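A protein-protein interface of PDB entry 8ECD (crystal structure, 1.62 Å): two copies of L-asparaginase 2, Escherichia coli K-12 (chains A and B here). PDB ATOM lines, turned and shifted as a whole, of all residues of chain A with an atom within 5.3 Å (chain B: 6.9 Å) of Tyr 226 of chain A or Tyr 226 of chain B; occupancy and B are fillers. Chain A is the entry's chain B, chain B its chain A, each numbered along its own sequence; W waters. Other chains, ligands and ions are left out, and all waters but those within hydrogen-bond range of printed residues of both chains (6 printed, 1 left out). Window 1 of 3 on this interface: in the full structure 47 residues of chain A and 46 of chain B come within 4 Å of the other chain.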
ATOM      1  N   ILE A 224      -5.452  23.973   8.734  1.00  0.00           N
ATOM      2  CA  ILE A 224      -6.856  23.496   8.936  1.00  0.00           C
ATOM      3  C   ILE A 224      -7.460  24.162  10.135  1.00  0.00           C
ATOM      4  O   ILE A 224      -6.835  24.157  11.185  1.00  0.00           O
ATOM      5  CB  ILE A 224      -6.875  21.944   9.026  1.00  0.00           C
ATOM      6  CG1 ILE A 224      -6.259  21.252   7.825  1.00  0.00           C
ATOM      7  CG2 ILE A 224      -8.322  21.507   9.303  1.00  0.00           C
ATOM      8  CD1 ILE A 224      -6.199  19.718   7.903  1.00  0.00           C
ATOM      9  N   VAL A 225      -8.683  24.713   9.955  1.00  0.00           N
ATOM     10  CA  VAL A 225      -9.441  25.304  11.062  1.00  0.00           C
ATOM     11  C   VAL A 225     -10.704  24.504  11.308  1.00  0.00           C
ATOM     12  O   VAL A 225     -11.277  23.978  10.380  1.00  0.00           O
ATOM     13  CB  VAL A 225      -9.774  26.784  10.816  1.00  0.00           C
ATOM     14  CG1 VAL A 225      -8.445  27.585  10.747  1.00  0.00           C
ATOM     15  CG2 VAL A 225     -10.600  26.991   9.571  1.00  0.00           C
ATOM     16  N   TYR A 226     -11.148  24.483  12.543  1.00  0.00           N
ATOM     17  CA  TYR A 226     -12.297  23.626  12.938  1.00  0.00           C
ATOM     18  C   TYR A 226     -13.475  24.545  13.207  1.00  0.00           C
ATOM     19  O   TYR A 226     -13.325  25.600  13.836  1.00  0.00           O
ATOM     20  CB  TYR A 226     -11.937  22.854  14.217  1.00  0.00           C
ATOM     21  CG  TYR A 226     -12.691  21.564  14.416  1.00  0.00           C
ATOM     22  CD1 TYR A 226     -12.380  20.450  13.646  1.00  0.00           C
ATOM     23  CD2 TYR A 226     -13.675  21.446  15.364  1.00  0.00           C
ATOM     24  CE1 TYR A 226     -13.085  19.254  13.800  1.00  0.00           C
ATOM     25  CE2 TYR A 226     -14.322  20.237  15.595  1.00  0.00           C
ATOM     26  CZ  TYR A 226     -14.021  19.137  14.815  1.00  0.00           C
ATOM     27  OH  TYR A 226     -14.655  17.939  15.008  1.00  0.00           O
ATOM     28  N   ASN A 227     -14.678  24.066  12.839  1.00  0.00           N
ATOM     29  CA  ASN A 227     -15.933  24.783  13.148  1.00  0.00           C
ATOM     30  C   ASN A 227     -16.730  24.003  14.184  1.00  0.00           C
ATOM     31  O   ASN A 227     -16.682  22.778  14.178  1.00  0.00           O
ATOM     32  CB  ASN A 227     -16.752  25.059  11.927  1.00  0.00           C
ATOM     33  CG  ASN A 227     -16.138  26.070  10.975  1.00  0.00           C
ATOM     34  OD1 ASN A 227     -16.558  27.210  10.941  1.00  0.00           O
ATOM     35  ND2 ASN A 227     -15.211  25.591  10.167  1.00  0.00           N
ATOM     36  N   TYR A 228     -17.450  24.787  14.990  1.00  0.00           N
ATOM     37  CA  TYR A 228     -18.270  24.265  16.100  1.00  0.00           C
ATOM     38  C   TYR A 228     -19.093  25.466  16.591  1.00  0.00           C
ATOM     39  O   TYR A 228     -18.925  26.574  16.060  1.00  0.00           O
ATOM     40  CB  TYR A 228     -17.369  23.686  17.193  1.00  0.00           C
ATOM     41  CG  TYR A 228     -16.281  24.622  17.657  1.00  0.00           C
ATOM     42  CD1 TYR A 228     -15.087  24.741  16.964  1.00  0.00           C
ATOM     43  CD2 TYR A 228     -16.448  25.393  18.790  1.00  0.00           C
ATOM     44  CE1 TYR A 228     -14.096  25.614  17.375  1.00  0.00           C
ATOM     45  CE2 TYR A 228     -15.467  26.270  19.219  1.00  0.00           C
ATOM     46  CZ  TYR A 228     -14.286  26.374  18.513  1.00  0.00           C
ATOM     47  OH  TYR A 228     -13.326  27.240  18.940  1.00  0.00           O
ATOM     48  N   ALA A 231     -17.601  29.229  17.514  1.00  0.00           N
ATOM     49  CA  ALA A 231     -16.214  29.035  17.092  1.00  0.00           C
ATOM     50  C   ALA A 231     -15.436  30.364  17.129  1.00  0.00           C
ATOM     51  O   ALA A 231     -15.896  31.338  16.608  1.00  0.00           O
ATOM     52  CB  ALA A 231     -16.129  28.476  15.710  1.00  0.00           C
ATOM     53  N   ALA A 250     -12.602  22.628   8.314  1.00  0.00           N
ATOM     54  CA  ALA A 250     -13.373  21.460   8.814  1.00  0.00           C
ATOM     55  C   ALA A 250     -14.722  22.031   9.242  1.00  0.00           C
ATOM     56  O   ALA A 250     -14.877  22.479  10.406  1.00  0.00           O
ATOM     57  CB  ALA A 250     -12.645  20.767   9.924  1.00  0.00           C
ATOM     58  N   VAL A 261     -15.899  32.820  11.450  1.00  0.00           N
ATOM     59  CA  VAL A 261     -14.934  32.058  10.614  1.00  0.00           C
ATOM     60  C   VAL A 261     -15.227  32.410   9.163  1.00  0.00           C
ATOM     61  O   VAL A 261     -14.335  32.589   8.354  1.00  0.00           O
ATOM     62  CB  VAL A 261     -15.007  30.534  10.909  1.00  0.00           C
ATOM     63  CG1 VAL A 261     -14.067  29.721  10.032  1.00  0.00           C
ATOM     64  CG2 VAL A 261     -14.642  30.255  12.367  1.00  0.00           C
ATOM     65  N   ARG A 280     -15.971  18.454   9.163  1.00  0.00           N
ATOM     66  CA  ARG A 280     -15.637  17.591  10.270  1.00  0.00           C
ATOM     67  C   ARG A 280     -16.480  16.311  10.286  1.00  0.00           C
ATOM     68  O   ARG A 280     -16.152  15.377  11.010  1.00  0.00           O
ATOM     69  CB  ARG A 280     -15.855  18.306  11.601  1.00  0.00           C
ATOM     70  CG  ARG A 280     -17.333  18.457  12.002  1.00  0.00           C
ATOM     71  CD  ARG A 280     -17.512  19.353  13.191  1.00  0.00           C
ATOM     72  NE  ARG A 280     -18.891  19.285  13.689  1.00  0.00           N
ATOM     73  CZ  ARG A 280     -19.348  19.942  14.746  1.00  0.00           C
ATOM     74  NH1 ARG A 280     -18.591  20.802  15.376  1.00  0.00           N
ATOM     75  NH2 ARG A 280     -20.553  19.675  15.206  1.00  0.00           N
ATOM     76  N   PRO A 307     -10.871  16.892   5.865  1.00  0.00           N
ATOM     77  CA  PRO A 307     -10.030  18.102   5.942  1.00  0.00           C
ATOM     78  C   PRO A 307      -8.545  17.802   5.637  1.00  0.00           C
ATOM     79  O   PRO A 307      -7.902  18.557   4.864  1.00  0.00           O
ATOM     80  CB  PRO A 307     -10.251  18.647   7.337  1.00  0.00           C
ATOM     81  CG  PRO A 307     -11.668  18.148   7.666  1.00  0.00           C
ATOM     82  CD  PRO A 307     -11.753  16.785   7.041  1.00  0.00           C
ATOM     83  N   GLN A 308      -8.028  16.706   6.224  1.00  0.00           N
ATOM     84  CA  GLN A 308      -6.584  16.365   6.102  1.00  0.00           C
ATOM     85  C   GLN A 308      -6.322  15.939   4.643  1.00  0.00           C
ATOM     86  O   GLN A 308      -5.189  16.187   4.153  1.00  0.00           O
ATOM     87  CB  GLN A 308      -6.150  15.410   7.198  1.00  0.00           C
ATOM     88  CG  GLN A 308      -6.923  14.062   7.241  1.00  0.00           C
ATOM     89  CD  GLN A 308      -8.130  14.135   8.149  1.00  0.00           C
ATOM     90  OE1 GLN A 308      -8.611  15.218   8.516  1.00  0.00           O
ATOM     91  NE2 GLN A 308      -8.627  12.949   8.559  1.00  0.00           N
ATOM     92  N   GLU B 102     -23.973  19.165  19.673  1.00  0.00           N
ATOM     93  CA  GLU B 102     -23.360  19.981  20.685  1.00  0.00           C
ATOM     94  C   GLU B 102     -24.420  20.531  21.638  1.00  0.00           C
ATOM     95  O   GLU B 102     -24.299  20.380  22.843  1.00  0.00           O
ATOM     96  CB  GLU B 102     -22.609  21.142  20.019  1.00  0.00           C
ATOM     97  CG  GLU B 102     -21.463  20.670  19.125  1.00  0.00           C
ATOM     98  CD  GLU B 102     -20.712  21.789  18.367  1.00  0.00           C
ATOM     99  OE1 GLU B 102     -20.365  22.769  18.989  1.00  0.00           O
ATOM    100  OE2 GLU B 102     -20.588  21.661  17.138  1.00  0.00           O
ATOM    101  N   ILE B 224     -10.906  24.841  19.812  1.00  0.00           N
ATOM    102  CA  ILE B 224     -10.543  23.516  19.273  1.00  0.00           C
ATOM    103  C   ILE B 224      -9.464  23.644  18.218  1.00  0.00           C
ATOM    104  O   ILE B 224      -9.629  24.461  17.307  1.00  0.00           O
ATOM    105  CB  ILE B 224     -11.776  22.769  18.720  1.00  0.00           C
ATOM    106  CG1 ILE B 224     -12.908  22.610  19.760  1.00  0.00           C
ATOM    107  CG2 ILE B 224     -11.346  21.434  18.135  1.00  0.00           C
ATOM    108  CD1 ILE B 224     -14.166  21.980  19.266  1.00  0.00           C
ATOM    109  N   VAL B 225      -8.388  22.865  18.333  1.00  0.00           N
ATOM    110  CA  VAL B 225      -7.318  22.838  17.313  1.00  0.00           C
ATOM    111  C   VAL B 225      -7.245  21.462  16.671  1.00  0.00           C
ATOM    112  O   VAL B 225      -7.470  20.475  17.342  1.00  0.00           O
ATOM    113  CB  VAL B 225      -5.962  23.223  17.915  1.00  0.00           C
ATOM    114  CG1 VAL B 225      -5.993  24.646  18.415  1.00  0.00           C
ATOM    115  CG2 VAL B 225      -5.524  22.328  19.041  1.00  0.00           C
ATOM    116  N   TYR B 226      -6.986  21.425  15.374  1.00  0.00           N
ATOM    117  CA  TYR B 226      -6.926  20.170  14.582  1.00  0.00           C
ATOM    118  C   TYR B 226      -5.447  19.723  14.452  1.00  0.00           C
ATOM    119  O   TYR B 226      -4.559  20.540  14.211  1.00  0.00           O
ATOM    120  CB  TYR B 226      -7.535  20.440  13.224  1.00  0.00           C
ATOM    121  CG  TYR B 226      -8.141  19.251  12.533  1.00  0.00           C
ATOM    122  CD1 TYR B 226      -9.309  18.696  13.011  1.00  0.00           C
ATOM    123  CD2 TYR B 226      -7.590  18.715  11.373  1.00  0.00           C
ATOM    124  CE1 TYR B 226      -9.912  17.638  12.366  1.00  0.00           C
ATOM    125  CE2 TYR B 226      -8.154  17.631  10.732  1.00  0.00           C
ATOM    126  CZ  TYR B 226      -9.375  17.129  11.199  1.00  0.00           C
ATOM    127  OH  TYR B 226     -10.026  16.072  10.579  1.00  0.00           O
ATOM    128  N   ASN B 227      -5.226  18.405  14.447  1.00  0.00           N
ATOM    129  CA  ASN B 227      -3.943  17.775  14.177  1.00  0.00           C
ATOM    130  C   ASN B 227      -3.984  16.996  12.877  1.00  0.00           C
ATOM    131  O   ASN B 227      -5.054  16.443  12.488  1.00  0.00           O
ATOM    132  CB  ASN B 227      -3.468  16.854  15.321  1.00  0.00           C
ATOM    133  CG  ASN B 227      -3.151  17.606  16.583  1.00  0.00           C
ATOM    134  OD1 ASN B 227      -1.968  17.868  16.875  1.00  0.00           O
ATOM    135  ND2 ASN B 227      -4.178  17.928  17.361  1.00  0.00           N
ATOM    136  N   TYR B 228      -2.846  16.955  12.190  1.00  0.00           N
ATOM    137  CA  TYR B 228      -2.673  16.429  10.837  1.00  0.00           C
ATOM    138  C   TYR B 228      -1.134  16.500  10.593  1.00  0.00           C
ATOM    139  O   TYR B 228      -0.381  17.020  11.444  1.00  0.00           O
ATOM    140  CB  TYR B 228      -3.478  17.201   9.817  1.00  0.00           C
ATOM    141  CG  TYR B 228      -3.205  18.706   9.826  1.00  0.00           C
ATOM    142  CD1 TYR B 228      -3.859  19.516  10.737  1.00  0.00           C
ATOM    143  CD2 TYR B 228      -2.352  19.297   8.926  1.00  0.00           C
ATOM    144  CE1 TYR B 228      -3.641  20.863  10.788  1.00  0.00           C
ATOM    145  CE2 TYR B 228      -2.106  20.660   8.964  1.00  0.00           C
ATOM    146  CZ  TYR B 228      -2.768  21.439   9.896  1.00  0.00           C
ATOM    147  OH  TYR B 228      -2.664  22.807  10.050  1.00  0.00           O
ATOM    148  N   ALA B 231       1.283  19.834  11.047  1.00  0.00           N
ATOM    149  CA  ALA B 231       0.314  20.757  11.627  1.00  0.00           C
ATOM    150  C   ALA B 231       1.014  22.050  12.112  1.00  0.00           C
ATOM    151  O   ALA B 231       1.978  21.973  12.840  1.00  0.00           O
ATOM    152  CB  ALA B 231      -0.426  20.139  12.738  1.00  0.00           C
ATOM    153  N   SER B 232       0.396  23.185  11.844  1.00  0.00           N
ATOM    154  CA  SER B 232       0.881  24.495  12.348  1.00  0.00           C
ATOM    155  C   SER B 232       0.560  24.622  13.825  1.00  0.00           C
ATOM    156  O   SER B 232      -0.557  24.240  14.260  1.00  0.00           O
ATOM    157  CB  SER B 232       0.220  25.637  11.648  1.00  0.00           C
ATOM    158  OG  SER B 232       0.688  26.910  12.118  1.00  0.00           O
ATOM    159  N   PRO B 235      -2.689  28.127  15.236  1.00  0.00           N
ATOM    160  CA  PRO B 235      -3.987  28.108  15.916  1.00  0.00           C
ATOM    161  C   PRO B 235      -3.927  27.980  17.444  1.00  0.00           C
ATOM    162  O   PRO B 235      -4.598  28.721  18.177  1.00  0.00           O
ATOM    163  CB  PRO B 235      -4.658  26.906  15.220  1.00  0.00           C
ATOM    164  CG  PRO B 235      -4.134  27.019  13.831  1.00  0.00           C
ATOM    165  CD  PRO B 235      -2.623  27.184  14.129  1.00  0.00           C
ATOM    166  N   VAL B 248      -9.301  22.244  23.409  1.00  0.00           N
ATOM    167  CA  VAL B 248      -9.519  20.822  23.052  1.00  0.00           C
ATOM    168  C   VAL B 248      -8.731  20.568  21.788  1.00  0.00           C
ATOM    169  O   VAL B 248      -8.832  21.304  20.797  1.00  0.00           O
ATOM    170  CB  VAL B 248     -11.011  20.514  22.814  1.00  0.00           C
ATOM    171  CG1 VAL B 248     -11.209  19.092  22.299  1.00  0.00           C
ATOM    172  CG2 VAL B 248     -11.829  20.777  24.045  1.00  0.00           C
ATOM    173  N   SER B 249      -7.944  19.512  21.823  1.00  0.00           N
ATOM    174  CA  SER B 249      -7.155  19.038  20.673  1.00  0.00           C
ATOM    175  C   SER B 249      -7.955  17.931  19.945  1.00  0.00           C
ATOM    176  O   SER B 249      -8.267  16.888  20.592  1.00  0.00           O
ATOM    177  CB  SER B 249      -5.877  18.460  21.152  1.00  0.00           C
ATOM    178  OG  SER B 249      -5.224  17.815  20.061  1.00  0.00           O
ATOM    179  N   ALA B 250      -8.218  18.130  18.679  1.00  0.00           N
ATOM    180  CA  ALA B 250      -8.710  17.076  17.752  1.00  0.00           C
ATOM    181  C   ALA B 250      -7.479  16.338  17.271  1.00  0.00           C
ATOM    182  O   ALA B 250      -6.870  16.740  16.261  1.00  0.00           O
ATOM    183  CB  ALA B 250      -9.517  17.652  16.617  1.00  0.00           C
ATOM    184  N   GLY B 251      -7.053  15.382  18.057  1.00  0.00           N
ATOM    185  CA  GLY B 251      -5.815  14.631  17.849  1.00  0.00           C
ATOM    186  C   GLY B 251      -5.898  13.680  16.661  1.00  0.00           C
ATOM    187  O   GLY B 251      -6.970  13.423  16.124  1.00  0.00           O
ATOM    188  N   VAL B 252      -4.772  13.119  16.306  1.00  0.00           N
ATOM    189  CA  VAL B 252      -4.739  12.032  15.286  1.00  0.00           C
ATOM    190  C   VAL B 252      -4.761  10.729  16.053  1.00  0.00           C
ATOM    191  O   VAL B 252      -4.193  10.612  17.191  1.00  0.00           O
ATOM    192  CB  VAL B 252      -3.541  12.167  14.339  1.00  0.00           C
ATOM    193  CG1 VAL B 252      -3.671  13.416  13.465  1.00  0.00           C
ATOM    194  CG2 VAL B 252      -2.203  12.137  15.047  1.00  0.00           C
ATOM    195  N   TYR B 258       0.597  16.478  16.942  1.00  0.00           N
ATOM    196  CA  TYR B 258       1.817  16.822  16.163  1.00  0.00           C
ATOM    197  C   TYR B 258       2.746  17.555  17.145  1.00  0.00           C
ATOM    198  O   TYR B 258       2.318  18.348  17.964  1.00  0.00           O
ATOM    199  CB  TYR B 258       1.414  17.685  14.992  1.00  0.00           C
ATOM    200  CG  TYR B 258       2.557  18.076  14.104  1.00  0.00           C
ATOM    201  CD1 TYR B 258       3.112  17.157  13.263  1.00  0.00           C
ATOM    202  CD2 TYR B 258       3.131  19.353  14.162  1.00  0.00           C
ATOM    203  CE1 TYR B 258       4.178  17.459  12.438  1.00  0.00           C
ATOM    204  CE2 TYR B 258       4.230  19.657  13.384  1.00  0.00           C
ATOM    205  CZ  TYR B 258       4.734  18.729  12.498  1.00  0.00           C
ATOM    206  OH  TYR B 258       5.792  18.977  11.618  1.00  0.00           O
ATOM    207  N   VAL B 261       2.316  21.270  18.019  1.00  0.00           N
ATOM    208  CA  VAL B 261       1.036  21.503  18.776  1.00  0.00           C
ATOM    209  C   VAL B 261       1.215  21.028  20.205  1.00  0.00           C
ATOM    210  O   VAL B 261       0.809  21.714  21.140  1.00  0.00           O
ATOM    211  CB  VAL B 261      -0.131  20.824  18.023  1.00  0.00           C
ATOM    212  CG1 VAL B 261      -1.420  20.976  18.797  1.00  0.00           C
ATOM    213  CG2 VAL B 261      -0.286  21.370  16.637  1.00  0.00           C
ATOM    214  N   SER B 279     -10.032  13.436  19.688  1.00  0.00           N
ATOM    215  CA  SER B 279      -9.548  12.814  18.441  1.00  0.00           C
ATOM    216  C   SER B 279     -10.406  13.299  17.265  1.00  0.00           C
ATOM    217  O   SER B 279     -11.668  13.315  17.409  1.00  0.00           O
ATOM    218  CB  SER B 279      -9.567  11.296  18.475  1.00  0.00           C
ATOM    219  OG  SER B 279      -9.095  10.812  17.232  1.00  0.00           O
ATOM    220  N   ARG B 280      -9.762  13.553  16.108  1.00  0.00           N
ATOM    221  CA  ARG B 280     -10.476  13.741  14.887  1.00  0.00           C
ATOM    222  C   ARG B 280     -11.114  12.436  14.364  1.00  0.00           C
ATOM    223  O   ARG B 280     -11.942  12.445  13.460  1.00  0.00           O
ATOM    224  CB  ARG B 280      -9.575  14.260  13.803  1.00  0.00           C
ATOM    225  CG  ARG B 280      -8.624  13.209  13.204  1.00  0.00           C
ATOM    226  CD  ARG B 280      -7.598  13.878  12.299  1.00  0.00           C
ATOM    227  NE  ARG B 280      -6.868  12.829  11.576  1.00  0.00           N
ATOM    228  CZ  ARG B 280      -5.910  13.067  10.672  1.00  0.00           C
ATOM    229  NH1 ARG B 280      -5.355  12.051   9.982  1.00  0.00           N
ATOM    230  NH2 ARG B 280      -5.441  14.307  10.508  1.00  0.00           N
ATOM    231  N   VAL B 281     -10.684  11.316  14.898  1.00  0.00           N
ATOM    232  CA  VAL B 281     -11.206   9.996  14.488  1.00  0.00           C
ATOM    233  C   VAL B 281     -12.635   9.824  15.008  1.00  0.00           C
ATOM    234  O   VAL B 281     -12.930  10.164  16.145  1.00  0.00           O
ATOM    235  CB  VAL B 281     -10.286   8.872  14.985  1.00  0.00           C
ATOM    236  CG1 VAL B 281     -10.816   7.504  14.719  1.00  0.00           C
ATOM    237  CG2 VAL B 281      -8.862   9.020  14.411  1.00  0.00           C
ATOM    238  N   ASN B 306     -16.094  13.423  21.285  1.00  0.00           N
ATOM    239  CA  ASN B 306     -15.417  14.004  20.119  1.00  0.00           C
ATOM    240  C   ASN B 306     -15.071  15.448  20.464  1.00  0.00           C
ATOM    241  O   ASN B 306     -15.415  15.952  21.545  1.00  0.00           O
ATOM    242  CB  ASN B 306     -16.280  13.788  18.871  1.00  0.00           C
ATOM    243  CG  ASN B 306     -17.568  14.568  18.841  1.00  0.00           C
ATOM    244  OD1 ASN B 306     -17.658  15.671  19.387  1.00  0.00           O
ATOM    245  ND2 ASN B 306     -18.587  14.045  18.153  1.00  0.00           N
ATOM    246  N   PRO B 307     -14.364  16.161  19.572  1.00  0.00           N
ATOM    247  CA  PRO B 307     -13.780  17.452  19.994  1.00  0.00           C
ATOM    248  C   PRO B 307     -14.842  18.458  20.443  1.00  0.00           C
ATOM    249  O   PRO B 307     -14.676  19.104  21.490  1.00  0.00           O
ATOM    250  CB  PRO B 307     -12.968  17.902  18.776  1.00  0.00           C
ATOM    251  CG  PRO B 307     -12.556  16.620  18.156  1.00  0.00           C
ATOM    252  CD  PRO B 307     -13.791  15.736  18.289  1.00  0.00           C
ATOM    253  N   GLN B 308     -15.926  18.554  19.661  1.00  0.00           N
ATOM    254  CA  GLN B 308     -17.006  19.555  19.913  1.00  0.00           C
ATOM    255  C   GLN B 308     -17.743  19.167  21.180  1.00  0.00           C
ATOM    256  O   GLN B 308     -18.218  20.050  21.894  1.00  0.00           O
ATOM    257  CB  GLN B 308     -17.834  19.763  18.638  1.00  0.00           C
ATOM    258  CG  GLN B 308     -18.516  18.504  18.091  1.00  0.00           C
ATOM    259  CD  GLN B 308     -17.663  17.768  17.085  1.00  0.00           C
ATOM    260  OE1 GLN B 308     -16.458  17.973  16.959  1.00  0.00           O
ATOM    261  NE2 GLN B 308     -18.265  16.905  16.268  1.00  0.00           N
HETATM  262  O   HOH W   1     -12.753  15.823  10.966  1.00  0.00           O
HETATM  263  O   HOH W   2      -6.755  24.134  13.889  1.00  0.00           O
HETATM  264  O   HOH W   3     -10.966  12.609  10.494  1.00  0.00           O
HETATM  265  O   HOH W   4     -16.986  15.342  14.033  1.00  0.00           O
HETATM  266  O   HOH W   5      -9.219  25.332  14.713  1.00  0.00           O
HETATM  267  O   HOH W   6     -14.663  12.964  11.972  1.00  0.00           O
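Tyr 226 of chain B touches Ile 224 of chain A.
CG2 of Ile 224 of chain B touches CD2 of Tyr 226 of chain A (3.6 Å).
Tyr 226 of chain B touches Tyr 226 of chain A (CD1 to CD1, 3.6 Å).
Tyr 228 of chain A touches Glu 102 of chain B.
Tyr 228 of chain A touches Ile 224 of chain B (OH to N, 3.5 Å).
Arg 280 of chain A touches Gln 308 of chain B (NH1 to CB, 3.5 Å).
Pro 307 of chain A touches Tyr 226 of chain B.
Of the printed residues of chain B, Tyr 226 of chain A touches Ile 224, Tyr 226 and Gln 308.
Of the printed residues of chain B, Arg 280 of chain A touches Glu 102 and Gln 308.
Of the printed residues of chain B, Pro 307 of chain A touches Tyr 226.
Of the printed residues of chain B, Gln 308 of chain A touches Tyr 226 and Arg 280.
Of the printed residues of chain A, Glu 102 of chain B touches Tyr 228 (3.6 Å) and Arg 280 (2.8 Å).
The nearest residue of chain A that does not touch Tyr 226 of chain B is Ala 250 of chain A (4.8 Å).
Ile 224 of chain A touches Tyr 226 of chain B, and with the chains exchanged Tyr 226 of chain A touches Ile 224 of chain B.
Ile 224 of chain A touches Tyr 228 of chain B, and with the chains exchanged Tyr 228 of chain A touches Ile 224 of chain B.
Tyr 226 of chain B touches its own counterpart, Tyr 226 of chain A.
Pro 307 of chain A touches Tyr 226 of chain B, but with the chains exchanged Tyr 226 of chain A does not touch Pro 307 of chain B (4.01 Å).
Positions printed for both chains: 224, 225, 226, 227, 228, 231, 250, 261, 280, 307 and 308.
Of the 12 pairs that touch across the chains among the printed residues, 9 have their exchanged pair printed and touching as well.
The side-chain amide oxygen (OD1) of Asn 306 of chain B lies close to the backbone NH (N) of Gln 308 of chain B (3.4 Å).
The guanidinium group (NH1) of Arg 280 of chain A lies within hydrogen-bond range of the backbone carbonyl oxygen (O) of Asn 227 of chain A, at 3.0 Å.
The backbone carbonyl oxygen (O) of Asn 227 of chain B sits at hydrogen-bond distance from the guanidinium group (NH2) of Arg 280 of chain B, 2.9 Å away.
The backbone carbonyl oxygen of Gly 251 of chain B is in hydrogen-bond range of the backbone NH of Arg 280 of chain B.
Water W2 bridges O of Ile 224 of chain A (2.7 Å) and N of Tyr 226 of chain B (3.1 Å).
Water W1 bridges OH of Tyr 226 of chain B and O of Arg 280 of chain A.
Water W5 bridges O of Ile 224 of chain B and N of Tyr 226 of chain A.
Water W6 lies within hydrogen-bond range of the backbone carbonyl oxygen of Arg 280 of chain A and the backbone carbonyl oxygen of Arg 280 of chain B.
Water W4 bridges NE2 of Gln 308 of chain B (3.0 Å) and O of Arg 280 of chain A (3.1 Å).
Water W3 bridges the side-chain amide nitrogen of Gln 308 of chain A (3.1 Å) and the backbone carbonyl oxygen of Arg 280 of chain B (3.1 Å).
The side-chain amide oxygen (OE1) of Gln 308 of chain A is in hydrogen-bond range of the side-chain hydroxyl (OH) of Tyr 226 of chain B.
The side-chain carboxylate (OE2) of Glu 102 of chain B lies within salt-bridge range of the guanidinium group (NH2) of Arg 280 of chain A (2.8 Å).
OH of Tyr 228 of chain B lies within hydrogen-bond range of N of Ile 224 of chain A (3.3 Å).
The side-chain amide oxygen of Gln 308 of chain B lies within hydrogen-bond range of the side-chain hydroxyl of Tyr 226 of chain A (2.7 Å).
NE of Arg 280 of chain B lies close to NE2 of Gln 308 of chain A (3.5 Å).
Of the 22 printed residues of chain B, 6 touch a printed residue of chain A.
Hydrophobic or aromatic side chains of chain B within 4 Å of the printed part of chain A: Ile 224, Tyr 226 and Tyr 228.
Along chain B the printed residues that touch a printed residue of chain A span positions 102 to 308.
Hydrophobic or aromatic side chains of chain A that line the printed part of chain B: Ile 224, Tyr 226, Tyr 228 and Pro 307.
Among the printed residues, 12 pairs touch across the chains.
Among the printed residues, Asp or Glu carboxylates within 4 Å of a Lys or Arg side-chain nitrogen of the other chain: Arg 280 of chain A with Glu 102 of chain B (2.8 Å).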
